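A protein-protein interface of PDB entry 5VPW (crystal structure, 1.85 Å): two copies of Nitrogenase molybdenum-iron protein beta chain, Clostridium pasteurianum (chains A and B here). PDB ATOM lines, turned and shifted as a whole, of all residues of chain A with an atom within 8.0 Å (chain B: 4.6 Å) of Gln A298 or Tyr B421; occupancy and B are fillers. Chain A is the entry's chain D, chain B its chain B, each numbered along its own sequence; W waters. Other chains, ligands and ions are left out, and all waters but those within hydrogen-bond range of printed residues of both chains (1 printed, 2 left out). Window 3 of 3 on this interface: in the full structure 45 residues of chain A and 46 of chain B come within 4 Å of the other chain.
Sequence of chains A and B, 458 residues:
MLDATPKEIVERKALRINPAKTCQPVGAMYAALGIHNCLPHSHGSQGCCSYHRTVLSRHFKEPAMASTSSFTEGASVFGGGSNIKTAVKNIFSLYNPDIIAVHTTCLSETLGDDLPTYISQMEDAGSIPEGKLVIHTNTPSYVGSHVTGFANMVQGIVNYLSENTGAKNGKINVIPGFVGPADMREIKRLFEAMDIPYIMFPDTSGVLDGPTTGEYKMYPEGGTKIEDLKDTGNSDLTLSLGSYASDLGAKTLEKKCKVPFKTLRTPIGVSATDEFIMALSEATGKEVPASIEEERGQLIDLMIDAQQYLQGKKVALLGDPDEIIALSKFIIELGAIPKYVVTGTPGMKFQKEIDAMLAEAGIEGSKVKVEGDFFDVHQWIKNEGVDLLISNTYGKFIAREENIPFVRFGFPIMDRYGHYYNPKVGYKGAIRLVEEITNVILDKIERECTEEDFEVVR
The side-chain carboxylate (OE2) of Glu A294 lies within salt-bridge range of the guanidinium group (NH2) of Arg B185, 2.9 Å away. NH2 of Arg B185 sits close to NE2 of Gln A298 (3.4 Å). The side-chain amide nitrogen (NE2) of Gln A298 lies within hydrogen-bond range of the backbone carbonyl oxygen (O) of Asp B209 (2.8 Å). The backbone carbonyl oxygen (O) of Gln A298 sits at hydrogen-bond distance from the side-chain hydroxyl (OH) of Tyr B421 (3.4 Å). ND2 of Asn B422 lies within hydrogen-bond range of OE2 of Glu A435 (2.8 Å). The side-chain carboxylate (OE2) of Glu A435 sits close to the backbone carbonyl oxygen (O) of Gly B418.
The guanidinium group of Arg B185 lies within salt-bridge range of the side-chain carboxylate of Asp B209. The backbone NH (N) of Gly B418 lies within hydrogen-bond range of the side-chain hydroxyl (OH) of Tyr B420, 3.3 Å away. The backbone carbonyl oxygen of Gly B418 lies within hydrogen-bond range of the side-chain amide nitrogen of Asn B422, 3.2 Å away.
Among the printed residues, merely in contact across the chains: Glu A294 with Pro B211, Gly A297 with Pro B211, Gln A298 with Pro B211, Asp A301 with Gly B210, Asp A301 with Tyr B421 and Ile A431 with Tyr B421.
Of the printed residues of chain B, Glu A294 touches Arg B185 (2.9 Å) and Pro B211 (3.9 Å). Of the printed residues of chain B, Gly A297 touches Pro B211. Ile A304 touches none of the printed residues of chain B. Lys A428 touches none of the printed residues of chain B. Printed residues of chain A within 4 Å of Asp B209: Gln A298 (2.8 Å). Printed residues of chain A within 4 Å of Pro B211: Glu A294 (3.9 Å), Gly A297 (3.4 Å) and Gln A298 (3.7 Å). Printed residues of chain A within 4 Å of Gly B418: Glu A435. Of the printed residues of chain A, Tyr B421 touches Gln A298 (3.4 Å), Asp A301 (3.8 Å) and Ile A431 (3.9 Å). The nearest residue of chain B that does not touch Gln A298 is Gly B210 (4.3 Å).
Printed residues of chain B that touch a printed residue of chain A: Arg B185, Asp B209, Gly B210, Pro B211, Gly B418, Tyr B421 and Asn B422. Hydrophobic or aromatic side chains of chain B within 4 Å of the printed part of chain A: Pro B211 and Tyr B421. Of the 20 printed residues of chain A, 6 touch a printed residue of chain B. Hydrophobic or aromatic side chains of chain A within 4 Å of the printed part of chain B: Ile A431. Among the printed residues, 12 pairs touch across the chains.
No position is printed for both chains.
Water W1 lies within hydrogen-bond range of the side-chain amide oxygen of Asn B422 (3.0 Å) and the side-chain carboxylate of Glu A435 (3.4 Å).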
ATOM      1  N   SER A 291      17.332 -27.902 -14.144  1.00  0.00           N
ATOM      2  CA  SER A 291      16.431 -27.419 -15.237  1.00  0.00           C
ATOM      3  C   SER A 291      15.259 -26.539 -14.770  1.00  0.00           C
ATOM      4  O   SER A 291      14.892 -25.575 -15.430  1.00  0.00           O
ATOM      5  CB  SER A 291      15.860 -28.587 -16.039  1.00  0.00           C
ATOM      6  OG  SER A 291      15.047 -29.383 -15.203  1.00  0.00           O
ATOM      7  N   ILE A 292      14.631 -26.941 -13.674  1.00  0.00           N
ATOM      8  CA  ILE A 292      13.558 -26.183 -13.054  1.00  0.00           C
ATOM      9  C   ILE A 292      14.086 -24.938 -12.389  1.00  0.00           C
ATOM     10  O   ILE A 292      13.475 -23.863 -12.484  1.00  0.00           O
ATOM     11  CB  ILE A 292      12.830 -27.055 -12.043  1.00  0.00           C
ATOM     12  CG1 ILE A 292      12.116 -28.192 -12.780  1.00  0.00           C
ATOM     13  CG2 ILE A 292      11.843 -26.251 -11.223  1.00  0.00           C
ATOM     14  CD1 ILE A 292      11.377 -29.097 -11.813  1.00  0.00           C
ATOM     15  N   GLU A 293      15.235 -25.044 -11.743  1.00  0.00           N
ATOM     16  CA  GLU A 293      15.833 -23.863 -11.148  1.00  0.00           C
ATOM     17  C   GLU A 293      16.200 -22.813 -12.227  1.00  0.00           C
ATOM     18  O   GLU A 293      15.973 -21.615 -12.027  1.00  0.00           O
ATOM     19  CB  GLU A 293      17.036 -24.209 -10.257  1.00  0.00           C
ATOM     20  CG  GLU A 293      17.637 -22.946  -9.618  1.00  0.00           C
ATOM     21  CD  GLU A 293      18.442 -23.165  -8.335  1.00  0.00           C
ATOM     22  OE1 GLU A 293      18.461 -24.296  -7.796  1.00  0.00           O
ATOM     23  OE2 GLU A 293      19.039 -22.168  -7.840  1.00  0.00           O
ATOM     24  N   GLU A 294      16.744 -23.262 -13.358  1.00  0.00           N
ATOM     25  CA  GLU A 294      17.080 -22.361 -14.457  1.00  0.00           C
ATOM     26  C   GLU A 294      15.795 -21.652 -15.005  1.00  0.00           C
ATOM     27  O   GLU A 294      15.803 -20.440 -15.267  1.00  0.00           O
ATOM     28  CB  GLU A 294      17.784 -23.109 -15.584  1.00  0.00           C
ATOM     29  CG  GLU A 294      18.271 -22.120 -16.630  1.00  0.00           C
ATOM     30  CD  GLU A 294      18.711 -22.730 -17.934  1.00  0.00           C
ATOM     31  OE1 GLU A 294      18.079 -23.688 -18.436  1.00  0.00           O
ATOM     32  OE2 GLU A 294      19.680 -22.190 -18.512  1.00  0.00           O
ATOM     33  N   GLU A 295      14.718 -22.420 -15.201  1.00  0.00           N
ATOM     34  CA  GLU A 295      13.437 -21.851 -15.655  1.00  0.00           C
ATOM     35  C   GLU A 295      12.924 -20.725 -14.741  1.00  0.00           C
ATOM     36  O   GLU A 295      12.481 -19.678 -15.214  1.00  0.00           O
ATOM     37  CB  GLU A 295      12.336 -22.915 -15.721  1.00  0.00           C
ATOM     38  CG  GLU A 295      12.455 -23.954 -16.805  1.00  0.00           C
ATOM     39  CD  GLU A 295      11.343 -25.039 -16.726  1.00  0.00           C
ATOM     40  OE1 GLU A 295      10.758 -25.370 -15.620  1.00  0.00           O
ATOM     41  OE2 GLU A 295      11.050 -25.588 -17.812  1.00  0.00           O
ATOM     42  N   ARG A 296      12.945 -20.959 -13.429  1.00  0.00           N
ATOM     43  CA  ARG A 296      12.533 -19.967 -12.485  1.00  0.00           C
ATOM     44  C   ARG A 296      13.391 -18.702 -12.595  1.00  0.00           C
ATOM     45  O   ARG A 296      12.857 -17.592 -12.604  1.00  0.00           O
ATOM     46  CB  ARG A 296      12.599 -20.528 -11.068  1.00  0.00           C
ATOM     47  CG  ARG A 296      12.193 -19.536 -10.011  1.00  0.00           C
ATOM     48  CD  ARG A 296      12.334 -20.159  -8.614  1.00  0.00           C
ATOM     49  NE  ARG A 296      11.703 -19.345  -7.587  1.00  0.00           N
ATOM     50  CZ  ARG A 296      12.208 -18.223  -7.097  1.00  0.00           C
ATOM     51  NH1 ARG A 296      13.374 -17.759  -7.532  1.00  0.00           N
ATOM     52  NH2 ARG A 296      11.515 -17.548  -6.189  1.00  0.00           N
ATOM     53  N   GLY A 297      14.705 -18.873 -12.666  1.00  0.00           N
ATOM     54  CA  GLY A 297      15.674 -17.742 -12.765  1.00  0.00           C
ATOM     55  C   GLY A 297      15.486 -16.985 -14.084  1.00  0.00           C
ATOM     56  O   GLY A 297      15.671 -15.771 -14.138  1.00  0.00           O
ATOM     57  N   GLN A 298      15.106 -17.688 -15.151  1.00  0.00           N
ATOM     58  CA  GLN A 298      14.715 -16.990 -16.405  1.00  0.00           C
ATOM     59  C   GLN A 298      13.443 -16.159 -16.252  1.00  0.00           C
ATOM     60  O   GLN A 298      13.331 -15.066 -16.846  1.00  0.00           O
ATOM     61  CB  GLN A 298      14.533 -17.980 -17.573  1.00  0.00           C
ATOM     62  CG  GLN A 298      15.839 -18.553 -18.107  1.00  0.00           C
ATOM     63  CD  GLN A 298      15.605 -19.692 -19.081  1.00  0.00           C
ATOM     64  OE1 GLN A 298      14.705 -20.506 -18.890  1.00  0.00           O
ATOM     65  NE2 GLN A 298      16.408 -19.745 -20.134  1.00  0.00           N
ATOM     66  N   LEU A 299      12.453 -16.698 -15.545  1.00  0.00           N
ATOM     67  CA  LEU A 299      11.249 -15.927 -15.217  1.00  0.00           C
ATOM     68  C   LEU A 299      11.607 -14.665 -14.415  1.00  0.00           C
ATOM     69  O   LEU A 299      11.145 -13.578 -14.708  1.00  0.00           O
ATOM     70  CB  LEU A 299      10.245 -16.786 -14.433  1.00  0.00           C
ATOM     71  CG  LEU A 299       9.035 -16.034 -13.896  1.00  0.00           C
ATOM     72  CD1 LEU A 299       8.230 -15.449 -15.058  1.00  0.00           C
ATOM     73  CD2 LEU A 299       8.180 -16.918 -13.033  1.00  0.00           C
ATOM     74  N   ILE A 300      12.423 -14.828 -13.394  1.00  0.00           N
ATOM     75  CA  ILE A 300      12.860 -13.698 -12.608  1.00  0.00           C
ATOM     76  C   ILE A 300      13.599 -12.681 -13.497  1.00  0.00           C
ATOM     77  O   ILE A 300      13.330 -11.493 -13.410  1.00  0.00           O
ATOM     78  CB  ILE A 300      13.747 -14.156 -11.434  1.00  0.00           C
ATOM     79  CG1 ILE A 300      12.962 -15.049 -10.461  1.00  0.00           C
ATOM     80  CG2 ILE A 300      14.388 -12.976 -10.717  1.00  0.00           C
ATOM     81  CD1 ILE A 300      11.727 -14.446  -9.846  1.00  0.00           C
ATOM     82  N   ASP A 301      14.495 -13.146 -14.369  1.00  0.00           N
ATOM     83  CA  ASP A 301      15.228 -12.262 -15.255  1.00  0.00           C
ATOM     84  C   ASP A 301      14.238 -11.430 -16.088  1.00  0.00           C
ATOM     85  O   ASP A 301      14.434 -10.235 -16.281  1.00  0.00           O
ATOM     86  CB  ASP A 301      16.136 -13.074 -16.190  1.00  0.00           C
ATOM     87  CG  ASP A 301      17.192 -12.221 -16.908  1.00  0.00           C
ATOM     88  OD1 ASP A 301      18.191 -11.810 -16.245  1.00  0.00           O
ATOM     89  OD2 ASP A 301      17.038 -11.997 -18.149  1.00  0.00           O
ATOM     90  N   LEU A 302      13.184 -12.069 -16.540  1.00  0.00           N
ATOM     91  CA  LEU A 302      12.187 -11.429 -17.400  1.00  0.00           C
ATOM     92  C   LEU A 302      11.371 -10.396 -16.643  1.00  0.00           C
ATOM     93  O   LEU A 302      11.097  -9.265 -17.139  1.00  0.00           O
ATOM     94  CB  LEU A 302      11.283 -12.515 -18.013  1.00  0.00           C
ATOM     95  CG  LEU A 302      10.171 -12.088 -18.981  1.00  0.00           C
ATOM     96  CD1 LEU A 302      10.710 -11.300 -20.159  1.00  0.00           C
ATOM     97  CD2 LEU A 302       9.399 -13.297 -19.500  1.00  0.00           C
ATOM     98  N   MET A 303      10.956 -10.761 -15.440  1.00  0.00           N
ATOM     99  CA  MET A 303      10.191  -9.881 -14.606  1.00  0.00           C
ATOM    100  C   MET A 303      10.972  -8.608 -14.264  1.00  0.00           C
ATOM    101  O   MET A 303      10.404  -7.509 -14.222  1.00  0.00           O
ATOM    102  CB  MET A 303       9.798 -10.608 -13.325  1.00  0.00           C
ATOM    103  CG  MET A 303       8.750 -11.694 -13.515  1.00  0.00           C
ATOM    104  SD  MET A 303       8.524 -12.690 -12.032  1.00  0.00           S
ATOM    105  CE  MET A 303       7.754 -11.574 -10.880  1.00  0.00           C
ATOM    106  N   ILE A 304      12.278  -8.755 -14.055  1.00  0.00           N
ATOM    107  CA  ILE A 304      13.144  -7.605 -13.860  1.00  0.00           C
ATOM    108  C   ILE A 304      13.423  -6.825 -15.165  1.00  0.00           C
ATOM    109  O   ILE A 304      13.312  -5.598 -15.211  1.00  0.00           O
ATOM    110  CB  ILE A 304      14.452  -8.039 -13.208  1.00  0.00           C
ATOM    111  CG1 ILE A 304      14.148  -8.516 -11.768  1.00  0.00           C
ATOM    112  CG2 ILE A 304      15.436  -6.878 -13.187  1.00  0.00           C
ATOM    113  CD1 ILE A 304      15.294  -9.262 -11.115  1.00  0.00           C
ATOM    114  N   ASP A 305      13.758  -7.538 -16.243  1.00  0.00           N
ATOM    115  CA  ASP A 305      14.023  -6.898 -17.534  1.00  0.00           C
ATOM    116  C   ASP A 305      12.825  -6.066 -18.004  1.00  0.00           C
ATOM    117  O   ASP A 305      13.002  -4.975 -18.530  1.00  0.00           O
ATOM    118  CB  ASP A 305      14.353  -7.957 -18.611  1.00  0.00           C
ATOM    119  CG  ASP A 305      15.759  -8.518 -18.486  1.00  0.00           C
ATOM    120  OD1 ASP A 305      16.592  -7.937 -17.741  1.00  0.00           O
ATOM    121  OD2 ASP A 305      16.054  -9.527 -19.172  1.00  0.00           O
ATOM    122  N   TYR A 427       6.773 -22.180 -14.169  1.00  0.00           N
ATOM    123  CA  TYR A 427       7.674 -21.084 -14.565  1.00  0.00           C
ATOM    124  C   TYR A 427       7.575 -20.843 -16.069  1.00  0.00           C
ATOM    125  O   TYR A 427       7.582 -19.718 -16.518  1.00  0.00           O
ATOM    126  CB  TYR A 427       9.127 -21.352 -14.138  1.00  0.00           C
ATOM    127  CG  TYR A 427       9.241 -21.682 -12.665  1.00  0.00           C
ATOM    128  CD1 TYR A 427       8.776 -20.788 -11.688  1.00  0.00           C
ATOM    129  CD2 TYR A 427       9.733 -22.910 -12.244  1.00  0.00           C
ATOM    130  CE1 TYR A 427       8.862 -21.100 -10.339  1.00  0.00           C
ATOM    131  CE2 TYR A 427       9.804 -23.244 -10.887  1.00  0.00           C
ATOM    132  CZ  TYR A 427       9.407 -22.344  -9.943  1.00  0.00           C
ATOM    133  OH  TYR A 427       9.456 -22.673  -8.605  1.00  0.00           O
ATOM    134  N   LYS A 428       7.423 -21.911 -16.833  1.00  0.00           N
ATOM    135  CA  LYS A 428       7.272 -21.814 -18.292  1.00  0.00           C
ATOM    136  C   LYS A 428       5.999 -21.053 -18.654  1.00  0.00           C
ATOM    137  O   LYS A 428       6.015 -20.146 -19.501  1.00  0.00           O
ATOM    138  CB  LYS A 428       7.169 -23.226 -18.838  1.00  0.00           C
ATOM    139  CG  LYS A 428       7.764 -23.470 -20.198  1.00  0.00           C
ATOM    140  CD  LYS A 428       7.457 -24.911 -20.622  1.00  0.00           C
ATOM    141  CE  LYS A 428       8.502 -25.479 -21.558  1.00  0.00           C
ATOM    142  NZ  LYS A 428       9.862 -25.293 -20.989  1.00  0.00           N
ATOM    143  N   ILE A 431       6.246 -17.282 -17.887  1.00  0.00           N
ATOM    144  CA  ILE A 431       7.018 -16.590 -18.923  1.00  0.00           C
ATOM    145  C   ILE A 431       6.066 -16.228 -20.065  1.00  0.00           C
ATOM    146  O   ILE A 431       6.063 -15.081 -20.519  1.00  0.00           O
ATOM    147  CB  ILE A 431       8.212 -17.431 -19.404  1.00  0.00           C
ATOM    148  CG1 ILE A 431       9.304 -17.426 -18.337  1.00  0.00           C
ATOM    149  CG2 ILE A 431       8.750 -16.902 -20.731  1.00  0.00           C
ATOM    150  CD1 ILE A 431      10.395 -18.445 -18.564  1.00  0.00           C
ATOM    151  N   ARG A 432       5.228 -17.176 -20.488  1.00  0.00           N
ATOM    152  CA  ARG A 432       4.273 -16.898 -21.570  1.00  0.00           C
ATOM    153  C   ARG A 432       3.304 -15.791 -21.182  1.00  0.00           C
ATOM    154  O   ARG A 432       2.963 -14.922 -22.011  1.00  0.00           O
ATOM    155  CB  ARG A 432       3.445 -18.140 -21.972  1.00  0.00           C
ATOM    156  CG  ARG A 432       4.260 -19.329 -22.477  1.00  0.00           C
ATOM    157  CD  ARG A 432       4.896 -19.100 -23.838  1.00  0.00           C
ATOM    158  NE  ARG A 432       4.136 -19.767 -24.889  1.00  0.00           N
ATOM    159  CZ  ARG A 432       3.219 -19.185 -25.645  1.00  0.00           C
ATOM    160  NH1 ARG A 432       2.915 -17.901 -25.477  1.00  0.00           N
ATOM    161  NH2 ARG A 432       2.612 -19.891 -26.582  1.00  0.00           N
ATOM    162  N   GLU A 435       5.122 -12.420 -21.343  1.00  0.00           N
ATOM    163  CA  GLU A 435       5.272 -12.045 -22.749  1.00  0.00           C
ATOM    164  C   GLU A 435       3.974 -11.442 -23.299  1.00  0.00           C
ATOM    165  O   GLU A 435       3.997 -10.390 -23.945  1.00  0.00           O
ATOM    166  CB  GLU A 435       5.685 -13.252 -23.590  1.00  0.00           C
ATOM    167  CG  GLU A 435       7.115 -13.720 -23.339  1.00  0.00           C
ATOM    168  CD  GLU A 435       7.476 -15.010 -24.084  1.00  0.00           C
ATOM    169  OE1 GLU A 435       6.597 -15.805 -24.512  1.00  0.00           O
ATOM    170  OE2 GLU A 435       8.668 -15.272 -24.183  1.00  0.00           O
ATOM    171  N   ALA B 182      17.003 -20.012 -28.061  1.00  0.00           N
ATOM    172  CA  ALA B 182      15.829 -20.876 -27.898  1.00  0.00           C
ATOM    173  C   ALA B 182      15.767 -21.950 -29.010  1.00  0.00           C
ATOM    174  O   ALA B 182      15.293 -23.068 -28.777  1.00  0.00           O
ATOM    175  CB  ALA B 182      14.552 -20.064 -27.904  1.00  0.00           C
ATOM    176  N   ARG B 185      18.260 -24.592 -28.186  1.00  0.00           N
ATOM    177  CA  ARG B 185      17.695 -25.449 -27.162  1.00  0.00           C
ATOM    178  C   ARG B 185      16.721 -26.446 -27.790  1.00  0.00           C
ATOM    179  O   ARG B 185      16.687 -27.604 -27.387  1.00  0.00           O
ATOM    180  CB  ARG B 185      16.979 -24.656 -26.054  1.00  0.00           C
ATOM    181  CG  ARG B 185      17.907 -23.994 -25.042  1.00  0.00           C
ATOM    182  CD  ARG B 185      17.090 -23.150 -24.080  1.00  0.00           C
ATOM    183  NE  ARG B 185      17.903 -22.293 -23.201  1.00  0.00           N
ATOM    184  CZ  ARG B 185      18.282 -22.615 -21.973  1.00  0.00           C
ATOM    185  NH1 ARG B 185      17.928 -23.774 -21.437  1.00  0.00           N
ATOM    186  NH2 ARG B 185      18.969 -21.755 -21.251  1.00  0.00           N
ATOM    187  N   ASP B 209      20.552 -16.263 -22.820  1.00  0.00           N
ATOM    188  CA  ASP B 209      19.156 -16.423 -22.385  1.00  0.00           C
ATOM    189  C   ASP B 209      19.096 -16.868 -20.931  1.00  0.00           C
ATOM    190  O   ASP B 209      18.214 -17.642 -20.528  1.00  0.00           O
ATOM    191  CB  ASP B 209      18.445 -17.426 -23.276  1.00  0.00           C
ATOM    192  CG  ASP B 209      19.039 -18.834 -23.166  1.00  0.00           C
ATOM    193  OD1 ASP B 209      20.098 -18.990 -22.510  1.00  0.00           O
ATOM    194  OD2 ASP B 209      18.460 -19.779 -23.743  1.00  0.00           O
ATOM    195  N   GLY B 210      20.028 -16.326 -20.150  1.00  0.00           N
ATOM    196  CA  GLY B 210      20.375 -16.866 -18.853  1.00  0.00           C
ATOM    197  C   GLY B 210      19.504 -16.332 -17.727  1.00  0.00           C
ATOM    198  O   GLY B 210      18.838 -15.305 -17.875  1.00  0.00           O
ATOM    199  N   PRO B 211      19.504 -17.040 -16.597  1.00  0.00           N
ATOM    200  CA  PRO B 211      18.734 -16.640 -15.427  1.00  0.00           C
ATOM    201  C   PRO B 211      19.354 -15.510 -14.647  1.00  0.00           C
ATOM    202  O   PRO B 211      20.528 -15.248 -14.799  1.00  0.00           O
ATOM    203  CB  PRO B 211      18.721 -17.910 -14.577  1.00  0.00           C
ATOM    204  CG  PRO B 211      20.009 -18.630 -14.950  1.00  0.00           C
ATOM    205  CD  PRO B 211      20.224 -18.313 -16.401  1.00  0.00           C
ATOM    206  N   GLY B 418      11.275 -11.382 -24.202  1.00  0.00           N
ATOM    207  CA  GLY B 418      11.068 -12.836 -24.117  1.00  0.00           C
ATOM    208  C   GLY B 418      11.212 -13.626 -25.399  1.00  0.00           C
ATOM    209  O   GLY B 418      11.193 -14.867 -25.369  1.00  0.00           O
ATOM    210  N   HIS B 419      11.360 -12.953 -26.537  1.00  0.00           N
ATOM    211  CA  HIS B 419      11.524 -13.648 -27.804  1.00  0.00           C
ATOM    212  C   HIS B 419      12.689 -14.672 -27.802  1.00  0.00           C
ATOM    213  O   HIS B 419      12.619 -15.705 -28.479  1.00  0.00           O
ATOM    214  CB  HIS B 419      11.682 -12.664 -28.977  1.00  0.00           C
ATOM    215  CG  HIS B 419      12.750 -11.637 -28.775  1.00  0.00           C
ATOM    216  ND1 HIS B 419      14.050 -11.832 -29.194  1.00  0.00           N
ATOM    217  CD2 HIS B 419      12.735 -10.432 -28.148  1.00  0.00           C
ATOM    218  CE1 HIS B 419      14.783 -10.778 -28.872  1.00  0.00           C
ATOM    219  NE2 HIS B 419      14.018  -9.919 -28.229  1.00  0.00           N
ATOM    220  N   TYR B 420      13.736 -14.366 -27.043  1.00  0.00           N
ATOM    221  CA  TYR B 420      14.896 -15.266 -26.852  1.00  0.00           C
ATOM    222  C   TYR B 420      14.565 -16.535 -26.037  1.00  0.00           C
ATOM    223  O   TYR B 420      15.406 -17.406 -25.943  1.00  0.00           O
ATOM    224  CB  TYR B 420      16.119 -14.503 -26.223  1.00  0.00           C
ATOM    225  CG  TYR B 420      15.667 -13.426 -25.263  1.00  0.00           C
ATOM    226  CD1 TYR B 420      15.301 -13.741 -23.995  1.00  0.00           C
ATOM    227  CD2 TYR B 420      15.449 -12.127 -25.704  1.00  0.00           C
ATOM    228  CE1 TYR B 420      14.803 -12.780 -23.149  1.00  0.00           C
ATOM    229  CE2 TYR B 420      14.936 -11.159 -24.890  1.00  0.00           C
ATOM    230  CZ  TYR B 420      14.621 -11.489 -23.603  1.00  0.00           C
ATOM    231  OH  TYR B 420      14.082 -10.566 -22.758  1.00  0.00           O
ATOM    232  N   TYR B 421      13.364 -16.633 -25.450  1.00  0.00           N
ATOM    233  CA  TYR B 421      12.844 -17.909 -24.891  1.00  0.00           C
ATOM    234  C   TYR B 421      11.901 -18.680 -25.812  1.00  0.00           C
ATOM    235  O   TYR B 421      11.395 -19.730 -25.423  1.00  0.00           O
ATOM    236  CB  TYR B 421      12.108 -17.694 -23.569  1.00  0.00           C
ATOM    237  CG  TYR B 421      12.901 -16.913 -22.528  1.00  0.00           C
ATOM    238  CD1 TYR B 421      14.206 -17.271 -22.209  1.00  0.00           C
ATOM    239  CD2 TYR B 421      12.330 -15.836 -21.849  1.00  0.00           C
ATOM    240  CE1 TYR B 421      14.928 -16.575 -21.267  1.00  0.00           C
ATOM    241  CE2 TYR B 421      13.050 -15.125 -20.903  1.00  0.00           C
ATOM    242  CZ  TYR B 421      14.350 -15.514 -20.618  1.00  0.00           C
ATOM    243  OH  TYR B 421      15.067 -14.818 -19.706  1.00  0.00           O
ATOM    244  N   ASN B 422      11.613 -18.147 -26.991  1.00  0.00           N
ATOM    245  CA  ASN B 422      10.571 -18.691 -27.871  1.00  0.00           C
ATOM    246  C   ASN B 422      11.228 -19.372 -29.077  1.00  0.00           C
ATOM    247  O   ASN B 422      11.804 -18.678 -29.926  1.00  0.00           O
ATOM    248  CB  ASN B 422       9.692 -17.535 -28.439  1.00  0.00           C
ATOM    249  CG  ASN B 422       9.020 -16.707 -27.354  1.00  0.00           C
ATOM    250  OD1 ASN B 422       8.421 -15.649 -27.645  1.00  0.00           O
ATOM    251  ND2 ASN B 422       9.072 -17.179 -26.128  1.00  0.00           N
ATOM    252  N   PRO B 423      11.145 -20.711 -29.180  1.00  0.00           N
ATOM    253  CA  PRO B 423      11.676 -21.295 -30.425  1.00  0.00           C
ATOM    254  C   PRO B 423      10.864 -20.913 -31.653  1.00  0.00           C
ATOM    255  O   PRO B 423       9.650 -20.753 -31.569  1.00  0.00           O
ATOM    256  CB  PRO B 423      11.559 -22.806 -30.175  1.00  0.00           C
ATOM    257  CG  PRO B 423      10.425 -22.933 -29.209  1.00  0.00           C
ATOM    258  CD  PRO B 423      10.543 -21.731 -28.306  1.00  0.00           C
HETATM  259  O   HOH W   1       6.489 -13.444 -27.009  1.00  0.00           O
